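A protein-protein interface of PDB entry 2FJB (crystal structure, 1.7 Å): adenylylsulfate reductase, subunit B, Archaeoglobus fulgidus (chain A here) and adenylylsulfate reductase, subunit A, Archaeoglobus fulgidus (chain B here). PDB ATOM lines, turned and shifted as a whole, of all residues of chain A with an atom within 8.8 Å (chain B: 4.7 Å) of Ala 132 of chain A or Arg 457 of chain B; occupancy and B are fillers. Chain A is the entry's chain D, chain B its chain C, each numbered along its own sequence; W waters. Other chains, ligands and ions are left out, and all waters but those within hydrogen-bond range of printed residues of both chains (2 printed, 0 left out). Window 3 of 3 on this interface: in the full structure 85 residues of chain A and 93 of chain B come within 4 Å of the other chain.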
ATOM      1  N   PRO A 114      -5.228 -22.686  25.587  1.00  0.00           N
ATOM      2  CA  PRO A 114      -5.437 -21.592  24.634  1.00  0.00           C
ATOM      3  C   PRO A 114      -4.245 -21.011  23.889  1.00  0.00           C
ATOM      4  O   PRO A 114      -4.306 -20.837  22.671  1.00  0.00           O
ATOM      5  CB  PRO A 114      -6.189 -20.544  25.463  1.00  0.00           C
ATOM      6  CG  PRO A 114      -5.762 -20.823  26.859  1.00  0.00           C
ATOM      7  CD  PRO A 114      -5.780 -22.329  26.906  1.00  0.00           C
ATOM      8  N   PHE A 115      -3.158 -20.727  24.596  1.00  0.00           N
ATOM      9  CA  PHE A 115      -2.000 -20.129  23.944  1.00  0.00           C
ATOM     10  C   PHE A 115      -0.754 -21.008  23.966  1.00  0.00           C
ATOM     11  O   PHE A 115       0.371 -20.507  23.963  1.00  0.00           O
ATOM     12  CB  PHE A 115      -1.721 -18.774  24.595  1.00  0.00           C
ATOM     13  CG  PHE A 115      -2.957 -17.928  24.759  1.00  0.00           C
ATOM     14  CD1 PHE A 115      -3.302 -17.408  26.003  1.00  0.00           C
ATOM     15  CD2 PHE A 115      -3.795 -17.684  23.674  1.00  0.00           C
ATOM     16  CE1 PHE A 115      -4.468 -16.657  26.168  1.00  0.00           C
ATOM     17  CE2 PHE A 115      -4.961 -16.936  23.827  1.00  0.00           C
ATOM     18  CZ  PHE A 115      -5.299 -16.422  25.075  1.00  0.00           C
ATOM     19  N   GLU A 116      -0.960 -22.321  23.964  1.00  0.00           N
ATOM     20  CA  GLU A 116       0.151 -23.267  23.988  1.00  0.00           C
ATOM     21  C   GLU A 116       1.151 -22.973  22.876  1.00  0.00           C
ATOM     22  O   GLU A 116       0.780 -22.877  21.706  1.00  0.00           O
ATOM     23  CB  GLU A 116      -0.366 -24.700  23.835  1.00  0.00           C
ATOM     24  CG  GLU A 116       0.721 -25.761  23.955  1.00  0.00           C
ATOM     25  CD  GLU A 116       0.188 -27.172  23.797  1.00  0.00           C
ATOM     26  OE1 GLU A 116      -0.192 -27.546  22.667  1.00  0.00           O
ATOM     27  OE2 GLU A 116       0.143 -27.905  24.806  1.00  0.00           O
ATOM     28  N   GLY A 117       2.416 -22.820  23.253  1.00  0.00           N
ATOM     29  CA  GLY A 117       3.455 -22.557  22.275  1.00  0.00           C
ATOM     30  C   GLY A 117       3.594 -21.119  21.800  1.00  0.00           C
ATOM     31  O   GLY A 117       4.563 -20.799  21.113  1.00  0.00           O
ATOM     32  N   PHE A 118       2.646 -20.253  22.157  1.00  0.00           N
ATOM     33  CA  PHE A 118       2.694 -18.849  21.736  1.00  0.00           C
ATOM     34  C   PHE A 118       3.688 -18.032  22.547  1.00  0.00           C
ATOM     35  O   PHE A 118       3.847 -18.243  23.749  1.00  0.00           O
ATOM     36  CB  PHE A 118       1.336 -18.154  21.915  1.00  0.00           C
ATOM     37  CG  PHE A 118       0.238 -18.670  21.032  1.00  0.00           C
ATOM     38  CD1 PHE A 118       0.447 -19.720  20.144  1.00  0.00           C
ATOM     39  CD2 PHE A 118      -1.036 -18.113  21.122  1.00  0.00           C
ATOM     40  CE1 PHE A 118      -0.601 -20.211  19.363  1.00  0.00           C
ATOM     41  CE2 PHE A 118      -2.086 -18.596  20.348  1.00  0.00           C
ATOM     42  CZ  PHE A 118      -1.865 -19.647  19.468  1.00  0.00           C
ATOM     43  N   PRO A 119       4.364 -17.072  21.903  1.00  0.00           N
ATOM     44  CA  PRO A 119       5.314 -16.252  22.653  1.00  0.00           C
ATOM     45  C   PRO A 119       4.481 -15.228  23.426  1.00  0.00           C
ATOM     46  O   PRO A 119       3.286 -15.086  23.172  1.00  0.00           O
ATOM     47  CB  PRO A 119       6.156 -15.611  21.555  1.00  0.00           C
ATOM     48  CG  PRO A 119       5.165 -15.456  20.431  1.00  0.00           C
ATOM     49  CD  PRO A 119       4.429 -16.778  20.459  1.00  0.00           C
ATOM     50  N   GLU A 120       5.090 -14.527  24.372  1.00  0.00           N
ATOM     51  CA  GLU A 120       4.350 -13.529  25.132  1.00  0.00           C
ATOM     52  C   GLU A 120       4.041 -12.325  24.249  1.00  0.00           C
ATOM     53  O   GLU A 120       4.790 -12.013  23.325  1.00  0.00           O
ATOM     54  CB  GLU A 120       5.158 -13.068  26.349  1.00  0.00           C
ATOM     55  CG  GLU A 120       5.366 -14.142  27.402  1.00  0.00           C
ATOM     56  CD  GLU A 120       4.060 -14.722  27.904  1.00  0.00           C
ATOM     57  OE1 GLU A 120       3.205 -13.945  28.382  1.00  0.00           O
ATOM     58  OE2 GLU A 120       3.887 -15.958  27.819  1.00  0.00           O
ATOM     59  N   PRO A 121       2.917 -11.644  24.507  1.00  0.00           N
ATOM     60  CA  PRO A 121       2.597 -10.476  23.684  1.00  0.00           C
ATOM     61  C   PRO A 121       3.542  -9.334  24.047  1.00  0.00           C
ATOM     62  O   PRO A 121       4.062  -9.283  25.161  1.00  0.00           O
ATOM     63  CB  PRO A 121       1.149 -10.176  24.064  1.00  0.00           C
ATOM     64  CG  PRO A 121       1.098 -10.591  25.504  1.00  0.00           C
ATOM     65  CD  PRO A 121       1.849 -11.907  25.488  1.00  0.00           C
ATOM     66  N   ALA A 125       4.506  -5.837  19.098  1.00  0.00           N
ATOM     67  CA  ALA A 125       3.617  -6.737  18.375  1.00  0.00           C
ATOM     68  C   ALA A 125       2.188  -6.198  18.331  1.00  0.00           C
ATOM     69  O   ALA A 125       1.467  -6.415  17.363  1.00  0.00           O
ATOM     70  CB  ALA A 125       3.630  -8.123  19.025  1.00  0.00           C
ATOM     71  N   SER A 128       1.184  -4.378  15.133  1.00  0.00           N
ATOM     72  CA  SER A 128       1.181  -5.059  13.841  1.00  0.00           C
ATOM     73  C   SER A 128      -0.192  -5.644  13.521  1.00  0.00           C
ATOM     74  O   SER A 128      -1.138  -5.502  14.292  1.00  0.00           O
ATOM     75  CB  SER A 128       2.209  -6.191  13.824  1.00  0.00           C
ATOM     76  OG  SER A 128       1.716  -7.331  14.510  1.00  0.00           O
ATOM     77  N   GLU A 129      -0.286  -6.312  12.376  1.00  0.00           N
ATOM     78  CA  GLU A 129      -1.534  -6.936  11.953  1.00  0.00           C
ATOM     79  C   GLU A 129      -1.628  -8.375  12.465  1.00  0.00           C
ATOM     80  O   GLU A 129      -2.654  -9.033  12.297  1.00  0.00           O
ATOM     81  CB  GLU A 129      -1.627  -6.953  10.424  1.00  0.00           C
ATOM     82  CG  GLU A 129      -1.634  -5.585   9.754  1.00  0.00           C
ATOM     83  CD  GLU A 129      -2.824  -4.736  10.158  1.00  0.00           C
ATOM     84  OE1 GLU A 129      -3.853  -5.309  10.573  1.00  0.00           O
ATOM     85  OE2 GLU A 129      -2.736  -3.495  10.047  1.00  0.00           O
ATOM     86  N   LEU A 130      -0.563  -8.857  13.099  1.00  0.00           N
ATOM     87  CA  LEU A 130      -0.521 -10.235  13.591  1.00  0.00           C
ATOM     88  C   LEU A 130      -1.375 -10.562  14.809  1.00  0.00           C
ATOM     89  O   LEU A 130      -1.378  -9.837  15.799  1.00  0.00           O
ATOM     90  CB  LEU A 130       0.922 -10.641  13.905  1.00  0.00           C
ATOM     91  CG  LEU A 130       1.949 -10.619  12.775  1.00  0.00           C
ATOM     92  CD1 LEU A 130       3.280 -11.156  13.295  1.00  0.00           C
ATOM     93  CD2 LEU A 130       1.461 -11.462  11.624  1.00  0.00           C
ATOM     94  N   LEU A 131      -2.089 -11.679  14.727  1.00  0.00           N
ATOM     95  CA  LEU A 131      -2.912 -12.145  15.832  1.00  0.00           C
ATOM     96  C   LEU A 131      -2.062 -13.149  16.600  1.00  0.00           C
ATOM     97  O   LEU A 131      -0.979 -13.523  16.153  1.00  0.00           O
ATOM     98  CB  LEU A 131      -4.175 -12.834  15.314  1.00  0.00           C
ATOM     99  CG  LEU A 131      -5.143 -11.959  14.515  1.00  0.00           C
ATOM    100  CD1 LEU A 131      -6.304 -12.814  14.034  1.00  0.00           C
ATOM    101  CD2 LEU A 131      -5.647 -10.802  15.384  1.00  0.00           C
ATOM    102  N   ALA A 132      -2.555 -13.595  17.748  1.00  0.00           N
ATOM    103  CA  ALA A 132      -1.820 -14.557  18.560  1.00  0.00           C
ATOM    104  C   ALA A 132      -1.454 -15.806  17.761  1.00  0.00           C
ATOM    105  O   ALA A 132      -2.290 -16.373  17.052  1.00  0.00           O
ATOM    106  CB  ALA A 132      -2.646 -14.940  19.784  1.00  0.00           C
ATOM    107  N   GLY A 133      -0.195 -16.222  17.878  1.00  0.00           N
ATOM    108  CA  GLY A 133       0.276 -17.411  17.184  1.00  0.00           C
ATOM    109  C   GLY A 133       0.731 -17.212  15.747  1.00  0.00           C
ATOM    110  O   GLY A 133       1.358 -18.101  15.165  1.00  0.00           O
ATOM    111  N   GLU A 134       0.430 -16.055  15.167  1.00  0.00           N
ATOM    112  CA  GLU A 134       0.814 -15.786  13.788  1.00  0.00           C
ATOM    113  C   GLU A 134       2.250 -15.302  13.666  1.00  0.00           C
ATOM    114  O   GLU A 134       2.812 -14.750  14.610  1.00  0.00           O
ATOM    115  CB  GLU A 134      -0.120 -14.752  13.168  1.00  0.00           C
ATOM    116  CG  GLU A 134      -1.577 -15.152  13.226  1.00  0.00           C
ATOM    117  CD  GLU A 134      -2.457 -14.209  12.449  1.00  0.00           C
ATOM    118  OE1 GLU A 134      -2.057 -13.038  12.269  1.00  0.00           O
ATOM    119  OE2 GLU A 134      -3.553 -14.637  12.032  1.00  0.00           O
ATOM    120  N   PRO A 135       2.845 -15.462  12.474  1.00  0.00           N
ATOM    121  CA  PRO A 135       2.203 -16.065  11.298  1.00  0.00           C
ATOM    122  C   PRO A 135       2.204 -17.592  11.214  1.00  0.00           C
ATOM    123  O   PRO A 135       1.513 -18.170  10.376  1.00  0.00           O
ATOM    124  CB  PRO A 135       2.972 -15.437  10.142  1.00  0.00           C
ATOM    125  CG  PRO A 135       4.357 -15.349  10.695  1.00  0.00           C
ATOM    126  CD  PRO A 135       4.129 -14.837  12.108  1.00  0.00           C
ATOM    127  N   GLU A 136       2.953 -18.251  12.087  1.00  0.00           N
ATOM    128  CA  GLU A 136       3.050 -19.702  12.023  1.00  0.00           C
ATOM    129  C   GLU A 136       1.791 -20.558  12.164  1.00  0.00           C
ATOM    130  O   GLU A 136       1.692 -21.602  11.514  1.00  0.00           O
ATOM    131  CB  GLU A 136       4.138 -20.171  12.983  1.00  0.00           C
ATOM    132  CG  GLU A 136       5.512 -19.762  12.476  1.00  0.00           C
ATOM    133  CD  GLU A 136       6.620 -20.024  13.466  1.00  0.00           C
ATOM    134  OE1 GLU A 136       6.726 -21.168  13.959  1.00  0.00           O
ATOM    135  OE2 GLU A 136       7.390 -19.079  13.738  1.00  0.00           O
ATOM    136  N   ILE A 137       0.824 -20.147  12.980  1.00  0.00           N
ATOM    137  CA  ILE A 137      -0.383 -20.960  13.097  1.00  0.00           C
ATOM    138  C   ILE A 137      -1.122 -21.015  11.761  1.00  0.00           C
ATOM    139  O   ILE A 137      -1.948 -21.898  11.534  1.00  0.00           O
ATOM    140  CB  ILE A 137      -1.358 -20.428  14.171  1.00  0.00           C
ATOM    141  CG1 ILE A 137      -1.733 -18.975  13.878  1.00  0.00           C
ATOM    142  CG2 ILE A 137      -0.742 -20.586  15.552  1.00  0.00           C
ATOM    143  CD1 ILE A 137      -2.834 -18.448  14.772  1.00  0.00           C
ATOM    144  N   ILE A 138      -0.822 -20.067  10.879  1.00  0.00           N
ATOM    145  CA  ILE A 138      -1.454 -20.017   9.565  1.00  0.00           C
ATOM    146  C   ILE A 138      -0.840 -21.085   8.656  1.00  0.00           C
ATOM    147  O   ILE A 138      -1.437 -21.487   7.654  1.00  0.00           O
ATOM    148  CB  ILE A 138      -1.279 -18.621   8.919  1.00  0.00           C
ATOM    149  CG1 ILE A 138      -1.875 -17.552   9.838  1.00  0.00           C
ATOM    150  CG2 ILE A 138      -1.964 -18.575   7.555  1.00  0.00           C
ATOM    151  CD1 ILE A 138      -1.616 -16.126   9.384  1.00  0.00           C
ATOM    152  N   GLY B  36     -14.378 -15.658  19.862  1.00  0.00           N
ATOM    153  CA  GLY B  36     -13.130 -15.325  19.200  1.00  0.00           C
ATOM    154  C   GLY B  36     -12.536 -14.070  19.814  1.00  0.00           C
ATOM    155  O   GLY B  36     -11.322 -13.963  19.992  1.00  0.00           O
ATOM    156  N   ALA B  37     -13.398 -13.111  20.140  1.00  0.00           N
ATOM    157  CA  ALA B  37     -12.956 -11.865  20.751  1.00  0.00           C
ATOM    158  C   ALA B  37     -12.445 -12.118  22.168  1.00  0.00           C
ATOM    159  O   ALA B  37     -11.422 -11.562  22.571  1.00  0.00           O
ATOM    160  CB  ALA B  37     -14.110 -10.844  20.776  1.00  0.00           C
ATOM    161  N   TYR B  39     -11.227 -14.906  23.375  1.00  0.00           N
ATOM    162  CA  TYR B  39      -9.981 -15.647  23.215  1.00  0.00           C
ATOM    163  C   TYR B  39      -8.796 -14.724  22.923  1.00  0.00           C
ATOM    164  O   TYR B  39      -7.797 -14.736  23.641  1.00  0.00           O
ATOM    165  CB  TYR B  39     -10.125 -16.661  22.069  1.00  0.00           C
ATOM    166  CG  TYR B  39      -8.833 -17.361  21.691  1.00  0.00           C
ATOM    167  CD1 TYR B  39      -8.330 -18.412  22.459  1.00  0.00           C
ATOM    168  CD2 TYR B  39      -8.107 -16.959  20.572  1.00  0.00           C
ATOM    169  CE1 TYR B  39      -7.134 -19.046  22.118  1.00  0.00           C
ATOM    170  CE2 TYR B  39      -6.912 -17.583  20.227  1.00  0.00           C
ATOM    171  CZ  TYR B  39      -6.433 -18.625  21.003  1.00  0.00           C
ATOM    172  OH  TYR B  39      -5.245 -19.234  20.659  1.00  0.00           O
ATOM    173  N   GLU B  40      -8.907 -13.928  21.863  1.00  0.00           N
ATOM    174  CA  GLU B  40      -7.827 -13.030  21.463  1.00  0.00           C
ATOM    175  C   GLU B  40      -7.593 -11.879  22.440  1.00  0.00           C
ATOM    176  O   GLU B  40      -6.453 -11.479  22.670  1.00  0.00           O
ATOM    177  CB  GLU B  40      -8.105 -12.470  20.061  1.00  0.00           C
ATOM    178  CG  GLU B  40      -6.922 -11.742  19.431  1.00  0.00           C
ATOM    179  CD  GLU B  40      -5.849 -12.686  18.913  1.00  0.00           C
ATOM    180  OE1 GLU B  40      -4.725 -12.216  18.637  1.00  0.00           O
ATOM    181  OE2 GLU B  40      -6.125 -13.895  18.767  1.00  0.00           O
ATOM    182  N   TYR B  43      -5.344 -12.723  25.340  1.00  0.00           N
ATOM    183  CA  TYR B  43      -3.927 -12.787  25.009  1.00  0.00           C
ATOM    184  C   TYR B  43      -3.254 -11.416  25.117  1.00  0.00           C
ATOM    185  O   TYR B  43      -2.265 -11.258  25.827  1.00  0.00           O
ATOM    186  CB  TYR B  43      -3.743 -13.330  23.591  1.00  0.00           C
ATOM    187  CG  TYR B  43      -2.302 -13.396  23.122  1.00  0.00           C
ATOM    188  CD1 TYR B  43      -1.450 -14.410  23.560  1.00  0.00           C
ATOM    189  CD2 TYR B  43      -1.795 -12.444  22.239  1.00  0.00           C
ATOM    190  CE1 TYR B  43      -0.125 -14.475  23.128  1.00  0.00           C
ATOM    191  CE2 TYR B  43      -0.470 -12.497  21.801  1.00  0.00           C
ATOM    192  CZ  TYR B  43       0.356 -13.515  22.250  1.00  0.00           C
ATOM    193  OH  TYR B  43       1.662 -13.578  21.817  1.00  0.00           O
ATOM    194  N   TRP B  44      -3.799 -10.420  24.424  1.00  0.00           N
ATOM    195  CA  TRP B  44      -3.208  -9.087  24.429  1.00  0.00           C
ATOM    196  C   TRP B  44      -3.469  -8.241  25.673  1.00  0.00           C
ATOM    197  O   TRP B  44      -2.671  -7.369  26.006  1.00  0.00           O
ATOM    198  CB  TRP B  44      -3.670  -8.302  23.193  1.00  0.00           C
ATOM    199  CG  TRP B  44      -3.341  -8.977  21.900  1.00  0.00           C
ATOM    200  CD1 TRP B  44      -4.172  -9.756  21.144  1.00  0.00           C
ATOM    201  CD2 TRP B  44      -2.077  -8.962  21.224  1.00  0.00           C
ATOM    202  NE1 TRP B  44      -3.504 -10.225  20.041  1.00  0.00           N
ATOM    203  CE2 TRP B  44      -2.216  -9.755  20.064  1.00  0.00           C
ATOM    204  CE3 TRP B  44      -0.840  -8.354  21.488  1.00  0.00           C
ATOM    205  CZ2 TRP B  44      -1.164  -9.961  19.164  1.00  0.00           C
ATOM    206  CZ3 TRP B  44       0.210  -8.557  20.592  1.00  0.00           C
ATOM    207  CH2 TRP B  44       0.040  -9.355  19.445  1.00  0.00           C
ATOM    208  N   GLY B 118      -5.449 -19.660  10.254  1.00  0.00           N
ATOM    209  CA  GLY B 118      -4.828 -19.874  11.549  1.00  0.00           C
ATOM    210  C   GLY B 118      -5.888 -20.282  12.550  1.00  0.00           C
ATOM    211  O   GLY B 118      -5.654 -21.131  13.410  1.00  0.00           O
ATOM    212  N   THR B 119      -7.065 -19.674  12.434  1.00  0.00           N
ATOM    213  CA  THR B 119      -8.171 -19.990  13.328  1.00  0.00           C
ATOM    214  C   THR B 119      -8.605 -21.447  13.144  1.00  0.00           C
ATOM    215  O   THR B 119      -8.791 -22.176  14.117  1.00  0.00           O
ATOM    216  CB  THR B 119      -9.371 -19.056  13.063  1.00  0.00           C
ATOM    217  OG1 THR B 119      -9.019 -17.716  13.434  1.00  0.00           O
ATOM    218  CG2 THR B 119     -10.587 -19.503  13.861  1.00  0.00           C
ATOM    219  N   LEU B 122      -6.223 -23.868  14.701  1.00  0.00           N
ATOM    220  CA  LEU B 122      -6.356 -23.906  16.153  1.00  0.00           C
ATOM    221  C   LEU B 122      -7.559 -24.774  16.515  1.00  0.00           C
ATOM    222  O   LEU B 122      -7.508 -25.559  17.463  1.00  0.00           O
ATOM    223  CB  LEU B 122      -6.545 -22.493  16.719  1.00  0.00           C
ATOM    224  CG  LEU B 122      -5.289 -21.617  16.790  1.00  0.00           C
ATOM    225  CD1 LEU B 122      -5.667 -20.177  17.130  1.00  0.00           C
ATOM    226  CD2 LEU B 122      -4.340 -22.181  17.838  1.00  0.00           C
ATOM    227  N   PHE B 453     -15.318 -16.077  14.058  1.00  0.00           N
ATOM    228  CA  PHE B 453     -14.429 -16.224  15.210  1.00  0.00           C
ATOM    229  C   PHE B 453     -13.208 -15.353  14.927  1.00  0.00           C
ATOM    230  O   PHE B 453     -12.723 -14.632  15.795  1.00  0.00           O
ATOM    231  CB  PHE B 453     -13.992 -17.684  15.353  1.00  0.00           C
ATOM    232  CG  PHE B 453     -13.185 -17.970  16.595  1.00  0.00           C
ATOM    233  CD1 PHE B 453     -13.803 -18.460  17.744  1.00  0.00           C
ATOM    234  CD2 PHE B 453     -11.803 -17.789  16.600  1.00  0.00           C
ATOM    235  CE1 PHE B 453     -13.055 -18.776  18.886  1.00  0.00           C
ATOM    236  CE2 PHE B 453     -11.040 -18.098  17.729  1.00  0.00           C
ATOM    237  CZ  PHE B 453     -11.669 -18.597  18.878  1.00  0.00           C
ATOM    238  N   THR B 454     -12.729 -15.408  13.690  1.00  0.00           N
ATOM    239  CA  THR B 454     -11.558 -14.637  13.298  1.00  0.00           C
ATOM    240  C   THR B 454     -11.772 -13.133  13.389  1.00  0.00           C
ATOM    241  O   THR B 454     -10.909 -12.417  13.894  1.00  0.00           O
ATOM    242  CB  THR B 454     -11.109 -15.006  11.873  1.00  0.00           C
ATOM    243  OG1 THR B 454     -10.756 -16.395  11.833  1.00  0.00           O
ATOM    244  CG2 THR B 454      -9.910 -14.167  11.455  1.00  0.00           C
ATOM    245  N   GLU B 455     -12.913 -12.645  12.908  1.00  0.00           N
ATOM    246  CA  GLU B 455     -13.185 -11.213  12.971  1.00  0.00           C
ATOM    247  C   GLU B 455     -13.244 -10.772  14.434  1.00  0.00           C
ATOM    248  O   GLU B 455     -12.881  -9.649  14.764  1.00  0.00           O
ATOM    249  CB  GLU B 455     -14.499 -10.874  12.246  1.00  0.00           C
ATOM    250  CG  GLU B 455     -14.812  -9.378  12.214  1.00  0.00           C
ATOM    251  CD  GLU B 455     -15.975  -9.032  11.295  1.00  0.00           C
ATOM    252  OE1 GLU B 455     -17.032  -9.684  11.397  1.00  0.00           O
ATOM    253  OE2 GLU B 455     -15.833  -8.099  10.475  1.00  0.00           O
ATOM    254  N   GLY B 456     -13.699 -11.666  15.306  1.00  0.00           N
ATOM    255  CA  GLY B 456     -13.755 -11.348  16.722  1.00  0.00           C
ATOM    256  C   GLY B 456     -12.339 -11.171  17.244  1.00  0.00           C
ATOM    257  O   GLY B 456     -12.069 -10.265  18.034  1.00  0.00           O
ATOM    258  N   ARG B 457     -11.429 -12.040  16.805  1.00  0.00           N
ATOM    259  CA  ARG B 457     -10.030 -11.958  17.219  1.00  0.00           C
ATOM    260  C   ARG B 457      -9.446 -10.620  16.765  1.00  0.00           C
ATOM    261  O   ARG B 457      -8.751  -9.944  17.521  1.00  0.00           O
ATOM    262  CB  ARG B 457      -9.206 -13.100  16.603  1.00  0.00           C
ATOM    263  CG  ARG B 457      -9.648 -14.507  16.988  1.00  0.00           C
ATOM    264  CD  ARG B 457      -8.767 -15.563  16.313  1.00  0.00           C
ATOM    265  NE  ARG B 457      -7.377 -15.470  16.759  1.00  0.00           N
ATOM    266  CZ  ARG B 457      -6.355 -16.098  16.182  1.00  0.00           C
ATOM    267  NH1 ARG B 457      -6.552 -16.878  15.126  1.00  0.00           N
ATOM    268  NH2 ARG B 457      -5.128 -15.936  16.657  1.00  0.00           N
ATOM    269  N   ILE B 458      -9.740 -10.241  15.525  1.00  0.00           N
ATOM    270  CA  ILE B 458      -9.232  -8.989  14.974  1.00  0.00           C
ATOM    271  C   ILE B 458      -9.706  -7.775  15.772  1.00  0.00           C
ATOM    272  O   ILE B 458      -8.910  -6.906  16.127  1.00  0.00           O
ATOM    273  CB  ILE B 458      -9.653  -8.834  13.496  1.00  0.00           C
ATOM    274  CG1 ILE B 458      -8.975  -9.923  12.654  1.00  0.00           C
ATOM    275  CG2 ILE B 458      -9.278  -7.448  12.987  1.00  0.00           C
ATOM    276  CD1 ILE B 458      -9.484 -10.012  11.214  1.00  0.00           C
ATOM    277  N   ALA B 459     -11.001  -7.720  16.063  1.00  0.00           N
ATOM    278  CA  ALA B 459     -11.552  -6.601  16.821  1.00  0.00           C
ATOM    279  C   ALA B 459     -10.981  -6.552  18.232  1.00  0.00           C
ATOM    280  O   ALA B 459     -10.722  -5.473  18.764  1.00  0.00           O
ATOM    281  CB  ALA B 459     -13.066  -6.710  16.887  1.00  0.00           C
ATOM    282  N   ALA B 460     -10.799  -7.726  18.829  1.00  0.00           N
ATOM    283  CA  ALA B 460     -10.270  -7.838  20.185  1.00  0.00           C
ATOM    284  C   ALA B 460      -8.875  -7.244  20.299  1.00  0.00           C
ATOM    285  O   ALA B 460      -8.585  -6.496  21.233  1.00  0.00           O
ATOM    286  CB  ALA B 460     -10.247  -9.299  20.614  1.00  0.00           C
ATOM    287  N   LYS B 461      -7.999  -7.579  19.360  1.00  0.00           N
ATOM    288  CA  LYS B 461      -6.655  -7.029  19.419  1.00  0.00           C
ATOM    289  C   LYS B 461      -6.721  -5.522  19.216  1.00  0.00           C
ATOM    290  O   LYS B 461      -6.010  -4.771  19.877  1.00  0.00           O
ATOM    291  CB  LYS B 461      -5.740  -7.630  18.352  1.00  0.00           C
ATOM    292  CG  LYS B 461      -4.328  -7.054  18.448  1.00  0.00           C
ATOM    293  CD  LYS B 461      -3.391  -7.543  17.362  1.00  0.00           C
ATOM    294  CE  LYS B 461      -2.011  -6.905  17.552  1.00  0.00           C
ATOM    295  NZ  LYS B 461      -1.032  -7.295  16.496  1.00  0.00           N
HETATM  296  O   HOH W   1      -4.864 -16.824  12.622  1.00  0.00           O
HETATM  297  O   HOH W   2       1.809 -14.686  19.059  1.00  0.00           O
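Along chain A the printed residues that touch a printed residue of chain B span positions 114 to 138.
Among the printed residues, no Asp or Glu carboxylate lies within 4 Å of a Lys or Arg side-chain nitrogen of the other chain.
Printed residues of chain B within 4 Å of Ala 125 of chain A: Trp 44 and Lys 461.
Of the printed residues of chain B, Leu 130 of chain A touches Trp 44 (3.4 Å) and Lys 461 (2.7 Å).
Of chain B, only Glu 40, Tyr 43 and Arg 457 come within 4 Å of Ala 132 of chain A.
Of the printed residues of chain B, Ile 137 of chain A touches Gly 118 (3.5 Å) and Arg 457 (3.9 Å).
Of the printed residues of chain A, Tyr 39 of chain B touches Pro 114 (2.7 Å), Phe 115 (3.3 Å) and Phe 118 (3.2 Å).
No residue of chain A comes within 4 Å of Gly 456 of chain B.
Of chain A, only Leu 131 (3.5 Å), Ala 132 (2.9 Å) and Ile 137 (3.9 Å) come within 4 Å of Arg 457 of chain B.
Ala 459 of chain B touches none of the printed residues of chain A.
Of the printed residues of chain A, Lys 461 of chain B touches Ala 125, Ser 128 and Leu 130.
The nearest printed residue of chain B that does not touch Pro 114 of chain A is Leu 122 of chain B (5.0 Å).
Water W1 lies within hydrogen-bond range of the side-chain carboxylate of Glu 134 of chain A (2.6 Å) and the guanidinium group of Arg 457 of chain B (3.0 Å).
Water W2 bridges the backbone NH of Gly 133 of chain A and the side-chain hydroxyl of Tyr 43 of chain B.
Among the printed residues, merely in contact across the chains: Phe 115 of chain A with Tyr 39 of chain B, Phe 115 of chain A with Tyr 43 of chain B, Phe 118 of chain A with Tyr 39 of chain B, Phe 118 of chain A with Leu 122 of chain B, Glu 120 of chain A with Tyr 43 of chain B, Pro 121 of chain A with Tyr 43 of chain B, Pro 121 of chain A with Trp 44 of chain B, Ala 125 of chain A with Trp 44 of chain B, Leu 130 of chain A with Trp 44 of chain B, Leu 131 of chain A with Glu 40 of chain B, Leu 131 of chain A with Arg 457 of chain B, Ala 132 of chain A with Tyr 43 of chain B, Ile 137 of chain A with Gly 118 of chain B, Ile 137 of chain A with Arg 457 of chain B and Ile 138 of chain A with Gly 118 of chain B.
O of Pro 114 of chain A sits at hydrogen-bond distance from OH of Tyr 39 of chain B (2.7 Å).
OE1 of Glu 40 of chain B is in hydrogen-bond range of N of Ala 132 of chain A.
The side-chain hydroxyl of Tyr 43 of chain B is in hydrogen-bond range of the backbone carbonyl oxygen of Pro 119 of chain A, at 2.6 Å.
The guanidinium group of Arg 457 of chain B lies within hydrogen-bond range of the backbone carbonyl oxygen of Ala 132 of chain A (2.9 Å).
The backbone carbonyl oxygen (O) of Ala 125 of chain A lies within hydrogen-bond range of the side-chain amino group (NZ) of Lys 461 of chain B (2.8 Å).
NZ of Lys 461 of chain B lies within hydrogen-bond range of O of Ser 128 of chain A, 2.8 Å away.
The backbone carbonyl oxygen (O) of Leu 130 of chain A sits at hydrogen-bond distance from the side-chain amino group (NZ) of Lys 461 of chain B, 2.7 Å away.
OE1 of Glu 40 of chain B sits at hydrogen-bond distance from NE1 of Trp 44 of chain B (2.7 Å).
The guanidinium group of Arg 457 of chain B lies within salt-bridge range of the side-chain carboxylate of Glu 40 of chain B (2.8 Å).
The guanidinium group (NH1) of Arg 457 of chain B sits at hydrogen-bond distance from the side-chain hydroxyl (OG1) of Thr 119 of chain B (3.1 Å).
The backbone carbonyl oxygen (O) of Ala 125 of chain A is in hydrogen-bond range of the side-chain hydroxyl (OG) of Ser 128 of chain A (3.0 Å).
The backbone NH (N) of Leu 130 of chain A sits at hydrogen-bond distance from the side-chain hydroxyl (OG) of Ser 128 of chain A (3.1 Å).
N of Leu 131 of chain A is in hydrogen-bond range of OE1 of Glu 134 of chain A.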
